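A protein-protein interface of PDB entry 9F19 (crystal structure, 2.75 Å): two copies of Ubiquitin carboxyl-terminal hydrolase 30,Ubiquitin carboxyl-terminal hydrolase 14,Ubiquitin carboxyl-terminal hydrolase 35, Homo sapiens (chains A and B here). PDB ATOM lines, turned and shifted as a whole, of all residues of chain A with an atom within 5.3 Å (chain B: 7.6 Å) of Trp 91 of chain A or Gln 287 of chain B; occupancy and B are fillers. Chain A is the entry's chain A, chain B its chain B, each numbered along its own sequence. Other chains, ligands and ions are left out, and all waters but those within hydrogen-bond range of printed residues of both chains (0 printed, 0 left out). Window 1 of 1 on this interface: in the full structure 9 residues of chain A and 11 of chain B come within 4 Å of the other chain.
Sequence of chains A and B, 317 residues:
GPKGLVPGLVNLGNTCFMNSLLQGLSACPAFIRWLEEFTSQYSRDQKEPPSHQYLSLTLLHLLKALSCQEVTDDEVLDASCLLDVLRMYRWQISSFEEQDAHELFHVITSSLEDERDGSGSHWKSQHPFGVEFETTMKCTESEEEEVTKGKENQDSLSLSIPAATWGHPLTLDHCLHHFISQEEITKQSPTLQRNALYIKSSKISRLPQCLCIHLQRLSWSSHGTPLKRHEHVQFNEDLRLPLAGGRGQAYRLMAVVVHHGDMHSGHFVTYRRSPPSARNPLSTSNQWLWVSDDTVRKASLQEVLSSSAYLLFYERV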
ATOM      1  N   LEU A  86      40.162  14.909  -8.774  1.00  0.00           N
ATOM      2  CA  LEU A  86      38.861  15.521  -8.520  1.00  0.00           C
ATOM      3  C   LEU A  86      38.686  16.860  -9.251  1.00  0.00           C
ATOM      4  O   LEU A  86      37.627  17.099  -9.906  1.00  0.00           O
ATOM      5  CB  LEU A  86      38.680  15.718  -7.015  1.00  0.00           C
ATOM      6  CG  LEU A  86      37.916  14.596  -6.359  1.00  0.00           C
ATOM      7  CD1 LEU A  86      37.962  14.823  -4.857  1.00  0.00           C
ATOM      8  CD2 LEU A  86      36.509  14.594  -6.926  1.00  0.00           C
ATOM      9  N   ARG A  87      39.710  17.737  -9.164  1.00  0.00           N
ATOM     10  CA  ARG A  87      39.661  19.013  -9.888  1.00  0.00           C
ATOM     11  C   ARG A  87      39.642  18.872 -11.404  1.00  0.00           C
ATOM     12  O   ARG A  87      38.994  19.657 -12.103  1.00  0.00           O
ATOM     13  CB  ARG A  87      40.944  19.812  -9.539  1.00  0.00           C
ATOM     14  CG  ARG A  87      40.882  20.546  -8.266  1.00  0.00           C
ATOM     15  CD  ARG A  87      41.931  21.650  -7.931  1.00  0.00           C
ATOM     16  NE  ARG A  87      43.301  21.164  -7.857  1.00  0.00           N
ATOM     17  CZ  ARG A  87      44.132  21.016  -8.885  1.00  0.00           C
ATOM     18  NH1 ARG A  87      43.828  21.457 -10.112  1.00  0.00           N
ATOM     19  NH2 ARG A  87      45.336  20.491  -8.662  1.00  0.00           N
ATOM     20  N   TYR A  89      38.357  16.526 -12.914  1.00  0.00           N
ATOM     21  CA  TYR A  89      36.970  16.190 -13.159  1.00  0.00           C
ATOM     22  C   TYR A  89      36.042  17.381 -12.931  1.00  0.00           C
ATOM     23  O   TYR A  89      34.830  17.164 -12.854  1.00  0.00           O
ATOM     24  CB  TYR A  89      36.556  15.023 -12.256  1.00  0.00           C
ATOM     25  CG  TYR A  89      36.663  13.657 -12.895  1.00  0.00           C
ATOM     26  CD1 TYR A  89      36.228  13.441 -14.196  1.00  0.00           C
ATOM     27  CD2 TYR A  89      37.207  12.580 -12.194  1.00  0.00           C
ATOM     28  CE1 TYR A  89      36.332  12.180 -14.791  1.00  0.00           C
ATOM     29  CE2 TYR A  89      37.315  11.318 -12.773  1.00  0.00           C
ATOM     30  CZ  TYR A  89      36.876  11.123 -14.076  1.00  0.00           C
ATOM     31  OH  TYR A  89      36.977   9.876 -14.665  1.00  0.00           O
ATOM     32  N   ARG A  90      36.591  18.603 -12.815  1.00  0.00           N
ATOM     33  CA  ARG A  90      35.830  19.848 -12.665  1.00  0.00           C
ATOM     34  C   ARG A  90      34.986  19.841 -11.395  1.00  0.00           C
ATOM     35  O   ARG A  90      33.822  20.249 -11.408  1.00  0.00           O
ATOM     36  CB  ARG A  90      34.972  20.149 -13.899  1.00  0.00           C
ATOM     37  N   TRP A  91      35.578  19.359 -10.296  1.00  0.00           N
ATOM     38  CA  TRP A  91      35.027  19.510  -8.950  1.00  0.00           C
ATOM     39  C   TRP A  91      35.744  20.664  -8.274  1.00  0.00           C
ATOM     40  O   TRP A  91      36.975  20.725  -8.288  1.00  0.00           O
ATOM     41  CB  TRP A  91      35.197  18.247  -8.105  1.00  0.00           C
ATOM     42  CG  TRP A  91      34.115  17.240  -8.296  1.00  0.00           C
ATOM     43  CD1 TRP A  91      34.151  16.132  -9.102  1.00  0.00           C
ATOM     44  CD2 TRP A  91      32.836  17.227  -7.659  1.00  0.00           C
ATOM     45  NE1 TRP A  91      32.959  15.444  -9.013  1.00  0.00           N
ATOM     46  CE2 TRP A  91      32.142  16.098  -8.128  1.00  0.00           C
ATOM     47  CE3 TRP A  91      32.204  18.070  -6.753  1.00  0.00           C
ATOM     48  CZ2 TRP A  91      30.850  15.801  -7.716  1.00  0.00           C
ATOM     49  CZ3 TRP A  91      30.923  17.764  -6.349  1.00  0.00           C
ATOM     50  CH2 TRP A  91      30.259  16.656  -6.838  1.00  0.00           C
ATOM     51  N   GLN A  92      34.981  21.583  -7.703  1.00  0.00           N
ATOM     52  CA  GLN A  92      35.583  22.734  -7.047  1.00  0.00           C
ATOM     53  C   GLN A  92      35.755  22.397  -5.582  1.00  0.00           C
ATOM     54  O   GLN A  92      34.876  22.669  -4.766  1.00  0.00           O
ATOM     55  CB  GLN A  92      34.722  23.971  -7.220  1.00  0.00           C
ATOM     56  CG  GLN A  92      35.490  25.245  -7.020  1.00  0.00           C
ATOM     57  CD  GLN A  92      34.731  26.442  -7.517  1.00  0.00           C
ATOM     58  OE1 GLN A  92      34.857  26.830  -8.684  1.00  0.00           O
ATOM     59  NE2 GLN A  92      33.915  27.029  -6.642  1.00  0.00           N
ATOM     60  N   ILE A  93      36.913  21.823  -5.239  1.00  0.00           N
ATOM     61  CA  ILE A  93      37.094  21.312  -3.884  1.00  0.00           C
ATOM     62  C   ILE A  93      37.159  22.420  -2.845  1.00  0.00           C
ATOM     63  O   ILE A  93      36.781  22.187  -1.691  1.00  0.00           O
ATOM     64  CB  ILE A  93      38.323  20.383  -3.801  1.00  0.00           C
ATOM     65  CG1 ILE A  93      39.509  20.831  -4.682  1.00  0.00           C
ATOM     66  CG2 ILE A  93      37.886  18.966  -4.147  1.00  0.00           C
ATOM     67  CD1 ILE A  93      40.304  22.094  -4.204  1.00  0.00           C
ATOM     68  N   PHE A  96      34.214  22.916  -0.581  1.00  0.00           N
ATOM     69  CA  PHE A  96      33.813  21.852   0.331  1.00  0.00           C
ATOM     70  C   PHE A  96      34.255  22.075   1.767  1.00  0.00           C
ATOM     71  O   PHE A  96      33.721  21.423   2.671  1.00  0.00           O
ATOM     72  CB  PHE A  96      34.348  20.508  -0.148  1.00  0.00           C
ATOM     73  CG  PHE A  96      33.495  19.888  -1.189  1.00  0.00           C
ATOM     74  CD1 PHE A  96      32.211  19.467  -0.873  1.00  0.00           C
ATOM     75  CD2 PHE A  96      33.957  19.740  -2.484  1.00  0.00           C
ATOM     76  CE1 PHE A  96      31.396  18.908  -1.830  1.00  0.00           C
ATOM     77  CE2 PHE A  96      33.150  19.184  -3.448  1.00  0.00           C
ATOM     78  CZ  PHE A  96      31.863  18.769  -3.118  1.00  0.00           C
ATOM     79  N   VAL A 107      30.769  12.521  -2.304  1.00  0.00           N
ATOM     80  CA  VAL A 107      31.241  12.842  -3.645  1.00  0.00           C
ATOM     81  C   VAL A 107      32.124  11.724  -4.183  1.00  0.00           C
ATOM     82  O   VAL A 107      31.994  11.327  -5.348  1.00  0.00           O
ATOM     83  CB  VAL A 107      31.944  14.211  -3.643  1.00  0.00           C
ATOM     84  CG1 VAL A 107      32.910  14.362  -4.812  1.00  0.00           C
ATOM     85  CG2 VAL A 107      30.895  15.285  -3.689  1.00  0.00           C
ATOM     86  N   SER A 110      29.866   8.777  -5.097  1.00  0.00           N
ATOM     87  CA  SER A 110      29.047   9.063  -6.273  1.00  0.00           C
ATOM     88  C   SER A 110      29.875   9.106  -7.542  1.00  0.00           C
ATOM     89  O   SER A 110      29.360   8.783  -8.619  1.00  0.00           O
ATOM     90  CB  SER A 110      28.323  10.388  -6.115  1.00  0.00           C
ATOM     91  OG  SER A 110      29.264  11.428  -5.917  1.00  0.00           O
ATOM     92  N   SER A 111      31.148   9.509  -7.435  1.00  0.00           N
ATOM     93  CA  SER A 111      32.066   9.493  -8.575  1.00  0.00           C
ATOM     94  C   SER A 111      32.589   8.094  -8.887  1.00  0.00           C
ATOM     95  O   SER A 111      32.865   7.786 -10.052  1.00  0.00           O
ATOM     96  CB  SER A 111      33.241  10.432  -8.326  1.00  0.00           C
ATOM     97  OG  SER A 111      32.815  11.775  -8.246  1.00  0.00           O
ATOM     98  N   ASP A 114      30.002   6.583 -11.015  1.00  0.00           N
ATOM     99  CA  ASP A 114      30.033   7.046 -12.400  1.00  0.00           C
ATOM    100  C   ASP A 114      31.004   6.238 -13.264  1.00  0.00           C
ATOM    101  O   ASP A 114      30.762   6.072 -14.466  1.00  0.00           O
ATOM    102  CB  ASP A 114      30.399   8.526 -12.457  1.00  0.00           C
ATOM    103  CG  ASP A 114      29.601   9.272 -13.499  1.00  0.00           C
ATOM    104  OD1 ASP A 114      28.550   8.742 -13.930  1.00  0.00           O
ATOM    105  OD2 ASP A 114      30.036  10.372 -13.901  1.00  0.00           O
ATOM    106  N   GLY B   4      32.522  14.120 -19.176  1.00  0.00           N
ATOM    107  CA  GLY B   4      31.176  14.191 -18.640  1.00  0.00           C
ATOM    108  C   GLY B   4      30.624  15.586 -18.483  1.00  0.00           C
ATOM    109  O   GLY B   4      29.578  15.757 -17.847  1.00  0.00           O
ATOM    110  N   LEU B   5      31.297  16.589 -19.029  1.00  0.00           N
ATOM    111  CA  LEU B   5      30.852  17.970 -18.948  1.00  0.00           C
ATOM    112  C   LEU B   5      29.951  18.320 -20.121  1.00  0.00           C
ATOM    113  O   LEU B   5      29.879  17.603 -21.128  1.00  0.00           O
ATOM    114  CB  LEU B   5      32.044  18.927 -18.925  1.00  0.00           C
ATOM    115  CG  LEU B   5      32.310  19.711 -17.646  1.00  0.00           C
ATOM    116  CD1 LEU B   5      32.263  18.776 -16.452  1.00  0.00           C
ATOM    117  CD2 LEU B   5      33.665  20.417 -17.770  1.00  0.00           C
ATOM    118  N   MET B 254      15.329  16.108 -13.732  1.00  0.00           N
ATOM    119  CA  MET B 254      16.378  16.311 -14.728  1.00  0.00           C
ATOM    120  C   MET B 254      17.137  17.621 -14.591  1.00  0.00           C
ATOM    121  O   MET B 254      18.352  17.637 -14.824  1.00  0.00           O
ATOM    122  CB  MET B 254      15.794  16.242 -16.135  1.00  0.00           C
ATOM    123  CG  MET B 254      15.402  14.840 -16.534  1.00  0.00           C
ATOM    124  SD  MET B 254      16.722  13.635 -16.284  1.00  0.00           S
ATOM    125  CE  MET B 254      15.816  12.118 -16.531  1.00  0.00           C
ATOM    126  N   ARG B 272      21.981  20.780 -13.777  1.00  0.00           N
ATOM    127  CA  ARG B 272      21.492  19.744 -14.677  1.00  0.00           C
ATOM    128  C   ARG B 272      22.340  18.479 -14.602  1.00  0.00           C
ATOM    129  O   ARG B 272      23.524  18.526 -14.283  1.00  0.00           O
ATOM    130  CB  ARG B 272      21.380  20.286 -16.113  1.00  0.00           C
ATOM    131  CG  ARG B 272      22.631  20.836 -16.760  1.00  0.00           C
ATOM    132  CD  ARG B 272      23.344  19.854 -17.600  1.00  0.00           C
ATOM    133  NE  ARG B 272      22.528  19.317 -18.677  1.00  0.00           N
ATOM    134  CZ  ARG B 272      22.609  19.700 -19.939  1.00  0.00           C
ATOM    135  NH1 ARG B 272      23.334  20.758 -20.285  1.00  0.00           N
ATOM    136  NH2 ARG B 272      21.908  19.030 -20.866  1.00  0.00           N
ATOM    137  N   ARG B 273      21.703  17.339 -14.876  1.00  0.00           N
ATOM    138  CA  ARG B 273      22.394  16.052 -14.923  1.00  0.00           C
ATOM    139  C   ARG B 273      23.385  16.008 -16.081  1.00  0.00           C
ATOM    140  O   ARG B 273      23.173  16.633 -17.120  1.00  0.00           O
ATOM    141  CB  ARG B 273      21.381  14.927 -15.094  1.00  0.00           C
ATOM    142  CG  ARG B 273      21.043  14.197 -13.849  1.00  0.00           C
ATOM    143  CD  ARG B 273      19.962  13.177 -14.112  1.00  0.00           C
ATOM    144  NE  ARG B 273      18.944  13.228 -13.075  1.00  0.00           N
ATOM    145  CZ  ARG B 273      19.008  12.515 -11.962  1.00  0.00           C
ATOM    146  NH1 ARG B 273      20.020  11.699 -11.728  1.00  0.00           N
ATOM    147  NH2 ARG B 273      18.043  12.638 -11.055  1.00  0.00           N
ATOM    148  N   SER B 274      24.458  15.241 -15.901  1.00  0.00           N
ATOM    149  CA  SER B 274      25.434  15.027 -16.961  1.00  0.00           C
ATOM    150  C   SER B 274      24.824  14.251 -18.134  1.00  0.00           C
ATOM    151  O   SER B 274      23.873  13.488 -17.948  1.00  0.00           O
ATOM    152  CB  SER B 274      26.627  14.262 -16.404  1.00  0.00           C
ATOM    153  OG  SER B 274      27.638  15.165 -16.028  1.00  0.00           O
ATOM    154  N   PRO B 275      25.327  14.453 -19.359  1.00  0.00           N
ATOM    155  CA  PRO B 275      24.805  13.690 -20.494  1.00  0.00           C
ATOM    156  C   PRO B 275      25.122  12.210 -20.348  1.00  0.00           C
ATOM    157  O   PRO B 275      26.143  11.840 -19.744  1.00  0.00           O
ATOM    158  CB  PRO B 275      25.548  14.294 -21.703  1.00  0.00           C
ATOM    159  CG  PRO B 275      26.116  15.567 -21.251  1.00  0.00           C
ATOM    160  CD  PRO B 275      26.357  15.417 -19.781  1.00  0.00           C
ATOM    161  N   THR B 284      20.520   6.995 -17.339  1.00  0.00           N
ATOM    162  CA  THR B 284      20.628   8.327 -16.755  1.00  0.00           C
ATOM    163  C   THR B 284      21.822   8.410 -15.802  1.00  0.00           C
ATOM    164  O   THR B 284      22.024   7.529 -14.961  1.00  0.00           O
ATOM    165  CB  THR B 284      19.322   8.679 -16.033  1.00  0.00           C
ATOM    166  OG1 THR B 284      18.213   8.123 -16.755  1.00  0.00           O
ATOM    167  CG2 THR B 284      19.138  10.171 -15.954  1.00  0.00           C
ATOM    168  N   SER B 285      22.629   9.461 -15.956  1.00  0.00           N
ATOM    169  CA  SER B 285      23.793   9.669 -15.101  1.00  0.00           C
ATOM    170  C   SER B 285      23.374  10.097 -13.693  1.00  0.00           C
ATOM    171  O   SER B 285      22.281  10.632 -13.470  1.00  0.00           O
ATOM    172  CB  SER B 285      24.724  10.721 -15.711  1.00  0.00           C
ATOM    173  OG  SER B 285      25.656  11.209 -14.754  1.00  0.00           O
ATOM    174  N   ASN B 286      24.262   9.849 -12.726  1.00  0.00           N
ATOM    175  CA  ASN B 286      24.034  10.304 -11.361  1.00  0.00           C
ATOM    176  C   ASN B 286      24.701  11.637 -11.043  1.00  0.00           C
ATOM    177  O   ASN B 286      24.423  12.213  -9.984  1.00  0.00           O
ATOM    178  CB  ASN B 286      24.456   9.214 -10.344  1.00  0.00           C
ATOM    179  CG  ASN B 286      25.988   8.966 -10.262  1.00  0.00           C
ATOM    180  OD1 ASN B 286      26.822   9.627 -10.897  1.00  0.00           O
ATOM    181  ND2 ASN B 286      26.347   7.962  -9.466  1.00  0.00           N
ATOM    182  N   GLN B 287      25.575  12.131 -11.923  1.00  0.00           N
ATOM    183  CA  GLN B 287      26.332  13.341 -11.633  1.00  0.00           C
ATOM    184  C   GLN B 287      25.569  14.589 -12.059  1.00  0.00           C
ATOM    185  O   GLN B 287      24.968  14.631 -13.138  1.00  0.00           O
ATOM    186  CB  GLN B 287      27.722  13.318 -12.297  1.00  0.00           C
ATOM    187  CG  GLN B 287      28.693  12.335 -11.631  1.00  0.00           C
ATOM    188  CD  GLN B 287      29.172  12.803 -10.246  1.00  0.00           C
ATOM    189  OE1 GLN B 287      28.947  13.950  -9.840  1.00  0.00           O
ATOM    190  NE2 GLN B 287      29.755  11.879  -9.482  1.00  0.00           N
ATOM    191  N   TRP B 288      25.617  15.609 -11.204  1.00  0.00           N
ATOM    192  CA  TRP B 288      24.974  16.888 -11.461  1.00  0.00           C
ATOM    193  C   TRP B 288      26.017  17.957 -11.769  1.00  0.00           C
ATOM    194  O   TRP B 288      27.157  17.897 -11.303  1.00  0.00           O
ATOM    195  CB  TRP B 288      24.110  17.315 -10.265  1.00  0.00           C
ATOM    196  CG  TRP B 288      22.901  16.441 -10.105  1.00  0.00           C
ATOM    197  CD1 TRP B 288      22.875  15.171  -9.607  1.00  0.00           C
ATOM    198  CD2 TRP B 288      21.546  16.754 -10.474  1.00  0.00           C
ATOM    199  NE1 TRP B 288      21.592  14.674  -9.631  1.00  0.00           N
ATOM    200  CE2 TRP B 288      20.755  15.624 -10.155  1.00  0.00           C
ATOM    201  CE3 TRP B 288      20.926  17.874 -11.045  1.00  0.00           C
ATOM    202  CZ2 TRP B 288      19.374  15.580 -10.384  1.00  0.00           C
ATOM    203  CZ3 TRP B 288      19.554  17.829 -11.273  1.00  0.00           C
ATOM    204  CH2 TRP B 288      18.791  16.686 -10.935  1.00  0.00           C
ATOM    205  N   LEU B 289      25.611  18.949 -12.559  1.00  0.00           N
ATOM    206  CA  LEU B 289      26.466  20.063 -12.937  1.00  0.00           C
ATOM    207  C   LEU B 289      25.793  21.385 -12.608  1.00  0.00           C
ATOM    208  O   LEU B 289      24.584  21.561 -12.810  1.00  0.00           O
ATOM    209  CB  LEU B 289      26.825  20.041 -14.433  1.00  0.00           C
ATOM    210  CG  LEU B 289      27.185  18.664 -14.983  1.00  0.00           C
ATOM    211  CD1 LEU B 289      27.112  18.659 -16.479  1.00  0.00           C
ATOM    212  CD2 LEU B 289      28.548  18.225 -14.505  1.00  0.00           C
ATOM    213  N   VAL B 296      31.002  25.992 -16.260  1.00  0.00           N
ATOM    214  CA  VAL B 296      30.380  24.708 -15.954  1.00  0.00           C
ATOM    215  C   VAL B 296      31.292  23.948 -14.995  1.00  0.00           C
ATOM    216  O   VAL B 296      32.515  23.911 -15.181  1.00  0.00           O
ATOM    217  CB  VAL B 296      30.070  23.913 -17.245  1.00  0.00           C
ATOM    218  CG1 VAL B 296      31.301  23.802 -18.169  1.00  0.00           C
ATOM    219  CG2 VAL B 296      29.496  22.539 -16.938  1.00  0.00           C
ATOM    220  N   ARG B 297      30.706  23.403 -13.933  1.00  0.00           N
ATOM    221  CA  ARG B 297      31.475  22.630 -12.963  1.00  0.00           C
ATOM    222  C   ARG B 297      30.589  21.536 -12.397  1.00  0.00           C
ATOM    223  O   ARG B 297      29.363  21.569 -12.544  1.00  0.00           O
ATOM    224  CB  ARG B 297      31.969  23.501 -11.821  1.00  0.00           C
ATOM    225  CG  ARG B 297      30.805  24.038 -11.014  1.00  0.00           C
ATOM    226  CD  ARG B 297      31.255  24.534  -9.698  1.00  0.00           C
ATOM    227  NE  ARG B 297      30.185  25.236  -9.012  1.00  0.00           N
ATOM    228  CZ  ARG B 297      29.390  24.678  -8.110  1.00  0.00           C
ATOM    229  NH1 ARG B 297      29.466  23.388  -7.822  1.00  0.00           N
ATOM    230  NH2 ARG B 297      28.506  25.436  -7.469  1.00  0.00           N
ATOM    231  N   LYS B 298      31.209  20.582 -11.706  1.00  0.00           N
ATOM    232  CA  LYS B 298      30.397  19.569 -11.049  1.00  0.00           C
ATOM    233  C   LYS B 298      29.648  20.179  -9.882  1.00  0.00           C
ATOM    234  O   LYS B 298      29.900  21.312  -9.461  1.00  0.00           O
ATOM    235  CB  LYS B 298      31.235  18.405 -10.534  1.00  0.00           C
ATOM    236  CG  LYS B 298      31.935  17.600 -11.603  1.00  0.00           C
ATOM    237  CD  LYS B 298      31.047  16.563 -12.253  1.00  0.00           C
ATOM    238  CE  LYS B 298      31.891  15.528 -12.968  1.00  0.00           C
ATOM    239  NZ  LYS B 298      32.428  16.021 -14.275  1.00  0.00           N
ATOM    240  N   ALA B 299      28.687  19.423  -9.383  1.00  0.00           N
ATOM    241  CA  ALA B 299      27.937  19.846  -8.216  1.00  0.00           C
ATOM    242  C   ALA B 299      27.401  18.587  -7.572  1.00  0.00           C
ATOM    243  O   ALA B 299      26.918  17.689  -8.269  1.00  0.00           O
ATOM    244  CB  ALA B 299      26.790  20.799  -8.572  1.00  0.00           C
ATOM    245  N   SER B 300      27.505  18.522  -6.253  1.00  0.00           N
ATOM    246  CA  SER B 300      26.972  17.382  -5.531  1.00  0.00           C
ATOM    247  C   SER B 300      25.450  17.409  -5.557  1.00  0.00           C
ATOM    248  O   SER B 300      24.823  18.419  -5.891  1.00  0.00           O
ATOM    249  CB  SER B 300      27.461  17.394  -4.092  1.00  0.00           C
ATOM    250  OG  SER B 300      27.401  18.721  -3.621  1.00  0.00           O
ATOM    251  N   LEU B 301      24.858  16.263  -5.213  1.00  0.00           N
ATOM    252  CA  LEU B 301      23.403  16.169  -5.186  1.00  0.00           C
ATOM    253  C   LEU B 301      22.818  17.055  -4.092  1.00  0.00           C
ATOM    254  O   LEU B 301      21.794  17.721  -4.305  1.00  0.00           O
ATOM    255  CB  LEU B 301      22.986  14.703  -5.010  1.00  0.00           C
ATOM    256  CG  LEU B 301      21.544  14.188  -5.209  1.00  0.00           C
ATOM    257  CD1 LEU B 301      20.633  14.340  -4.004  1.00  0.00           C
ATOM    258  CD2 LEU B 301      20.922  14.883  -6.393  1.00  0.00           C
ATOM    259  N   GLU B 303      23.899  19.818  -2.983  1.00  0.00           N
ATOM    260  CA  GLU B 303      23.892  21.202  -3.436  1.00  0.00           C
ATOM    261  C   GLU B 303      22.651  21.471  -4.290  1.00  0.00           C
ATOM    262  O   GLU B 303      21.995  22.515  -4.128  1.00  0.00           O
ATOM    263  CB  GLU B 303      25.191  21.494  -4.198  1.00  0.00           C
ATOM    264  CG  GLU B 303      25.338  22.939  -4.660  1.00  0.00           C
ATOM    265  CD  GLU B 303      26.620  23.199  -5.471  1.00  0.00           C
ATOM    266  OE1 GLU B 303      27.433  22.250  -5.662  1.00  0.00           O
ATOM    267  OE2 GLU B 303      26.799  24.363  -5.919  1.00  0.00           O
ATOM    268  N   VAL B 304      22.275  20.499  -5.137  1.00  0.00           N
ATOM    269  CA  VAL B 304      21.109  20.652  -6.006  1.00  0.00           C
ATOM    270  C   VAL B 304      19.821  20.653  -5.188  1.00  0.00           C
ATOM    271  O   VAL B 304      18.931  21.491  -5.392  1.00  0.00           O
ATOM    272  CB  VAL B 304      21.082  19.546  -7.075  1.00  0.00           C
ATOM    273  CG1 VAL B 304      19.801  19.626  -7.897  1.00  0.00           C
ATOM    274  CG2 VAL B 304      22.271  19.649  -7.993  1.00  0.00           C
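Of the 21 printed residues of chain B, 8 touch a printed residue of chain A. Hydrophobic or aromatic side chains of chain B that line the printed part of chain A: Leu 5. Printed residues of chain A that touch a printed residue of chain B: Tyr 89, Arg 90, Trp 91, Ser 110, Ser 111 and Asp 114. Hydrophobic or aromatic side chains of chain A within 4 Å of the printed part of chain B: Trp 91. Along chain A the printed residues that touch a printed residue of chain B span positions 89 to 114. Among the printed residues, 14 pairs touch across the chains. Among the printed residues, no Asp or Glu carboxylate lies within 4 Å of a Lys or Arg side-chain nitrogen of the other chain.
OG of Ser 110 of chain A sits at hydrogen-bond distance from O of Val 107 of chain A, 2.8 Å away. The backbone carbonyl oxygen (O) of Ser 285 of chain B is in hydrogen-bond range of the guanidinium group (NH1) of Arg 273 of chain B (3.0 Å). N of Ser 274 of chain B is in hydrogen-bond range of O of Gln 287 of chain B (2.9 Å). The side-chain hydroxyl of Ser 285 of chain B is in hydrogen-bond range of the backbone NH of Gln 287 of chain B, 3.0 Å away. The backbone NH (N) of Ala 299 of chain B sits at hydrogen-bond distance from the backbone carbonyl oxygen (O) of Trp 288 of chain B (2.9 Å). The guanidinium group (NH2) of Arg 297 of chain B lies within salt-bridge range of the side-chain carboxylate (OE2) of Glu 303 of chain B (2.5 Å).
Of chain B, only Gln 287, Lys 298, Ala 299 and Ser 300 come within 4 Å of Trp 91 of chain A. Gln 287 of chain B touches just these residues of chain A: Trp 91 (3.4 Å), Ser 110 (3.2 Å), Ser 111 (3.3 Å) and Asp 114 (3.3 Å). Of the printed residues of chain B, Asp 114 of chain A touches Ser 285 (3.9 Å), Asn 286 (3.6 Å) and Gln 287 (3.3 Å). Of the printed residues of chain A, Ser 300 of chain B touches Trp 91. Printed residues of chain A within 4 Å of Lys 298 of chain B: Tyr 89 (3.0 Å), Arg 90 (2.7 Å) and Trp 91 (3.5 Å). Of the printed residues of chain B, Ser 111 of chain A touches Gln 287 (3.3 Å). Met 254 of chain B touches none of the printed residues of chain A. Thr 284 of chain B touches none of the printed residues of chain A. The nearest residue of chain B that does not touch Trp 91 of chain A is Trp 288 of chain B (5.6 Å).
No position is printed for both chains. Of the 14 pairs that touch across the chains among the printed residues, none has its exchanged pair printed and touching as well.
Among the printed residues, merely in contact across the chains: Asp 114 of chain A with Gln 287 of chain B, Trp 91 of chain A with Ser 300 of chain B, Trp 91 of chain A with Gln 287 of chain B, Trp 91 of chain A with Lys 298 of chain B, Trp 91 of chain A with Ala 299 of chain B, Asp 114 of chain A with Asn 286 of chain B, Arg 90 of chain A with Arg 297 of chain B, Asp 114 of chain A with Ser 285 of chain B and Arg 90 of chain A with Leu 5 of chain B.
The backbone carbonyl oxygen (O) of Tyr 89 of chain A lies within hydrogen-bond range of the side-chain amino group (NZ) of Lys 298 of chain B. The backbone NH of Lys 298 of chain B is in hydrogen-bond range of the backbone carbonyl oxygen of Arg 90 of chain A, 2.7 Å away. The backbone carbonyl oxygen of Ser 110 of chain A lies within hydrogen-bond range of the side-chain amide nitrogen of Asn 286 of chain B, at 3.2 Å. The backbone carbonyl oxygen (O) of Ser 110 of chain A sits at hydrogen-bond distance from the side-chain amide nitrogen (NE2) of Gln 287 of chain B. The side-chain hydroxyl (OG) of Ser 111 of chain A is in hydrogen-bond range of the side-chain amide nitrogen (NE2) of Gln 287 of chain B, 3.3 Å away.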
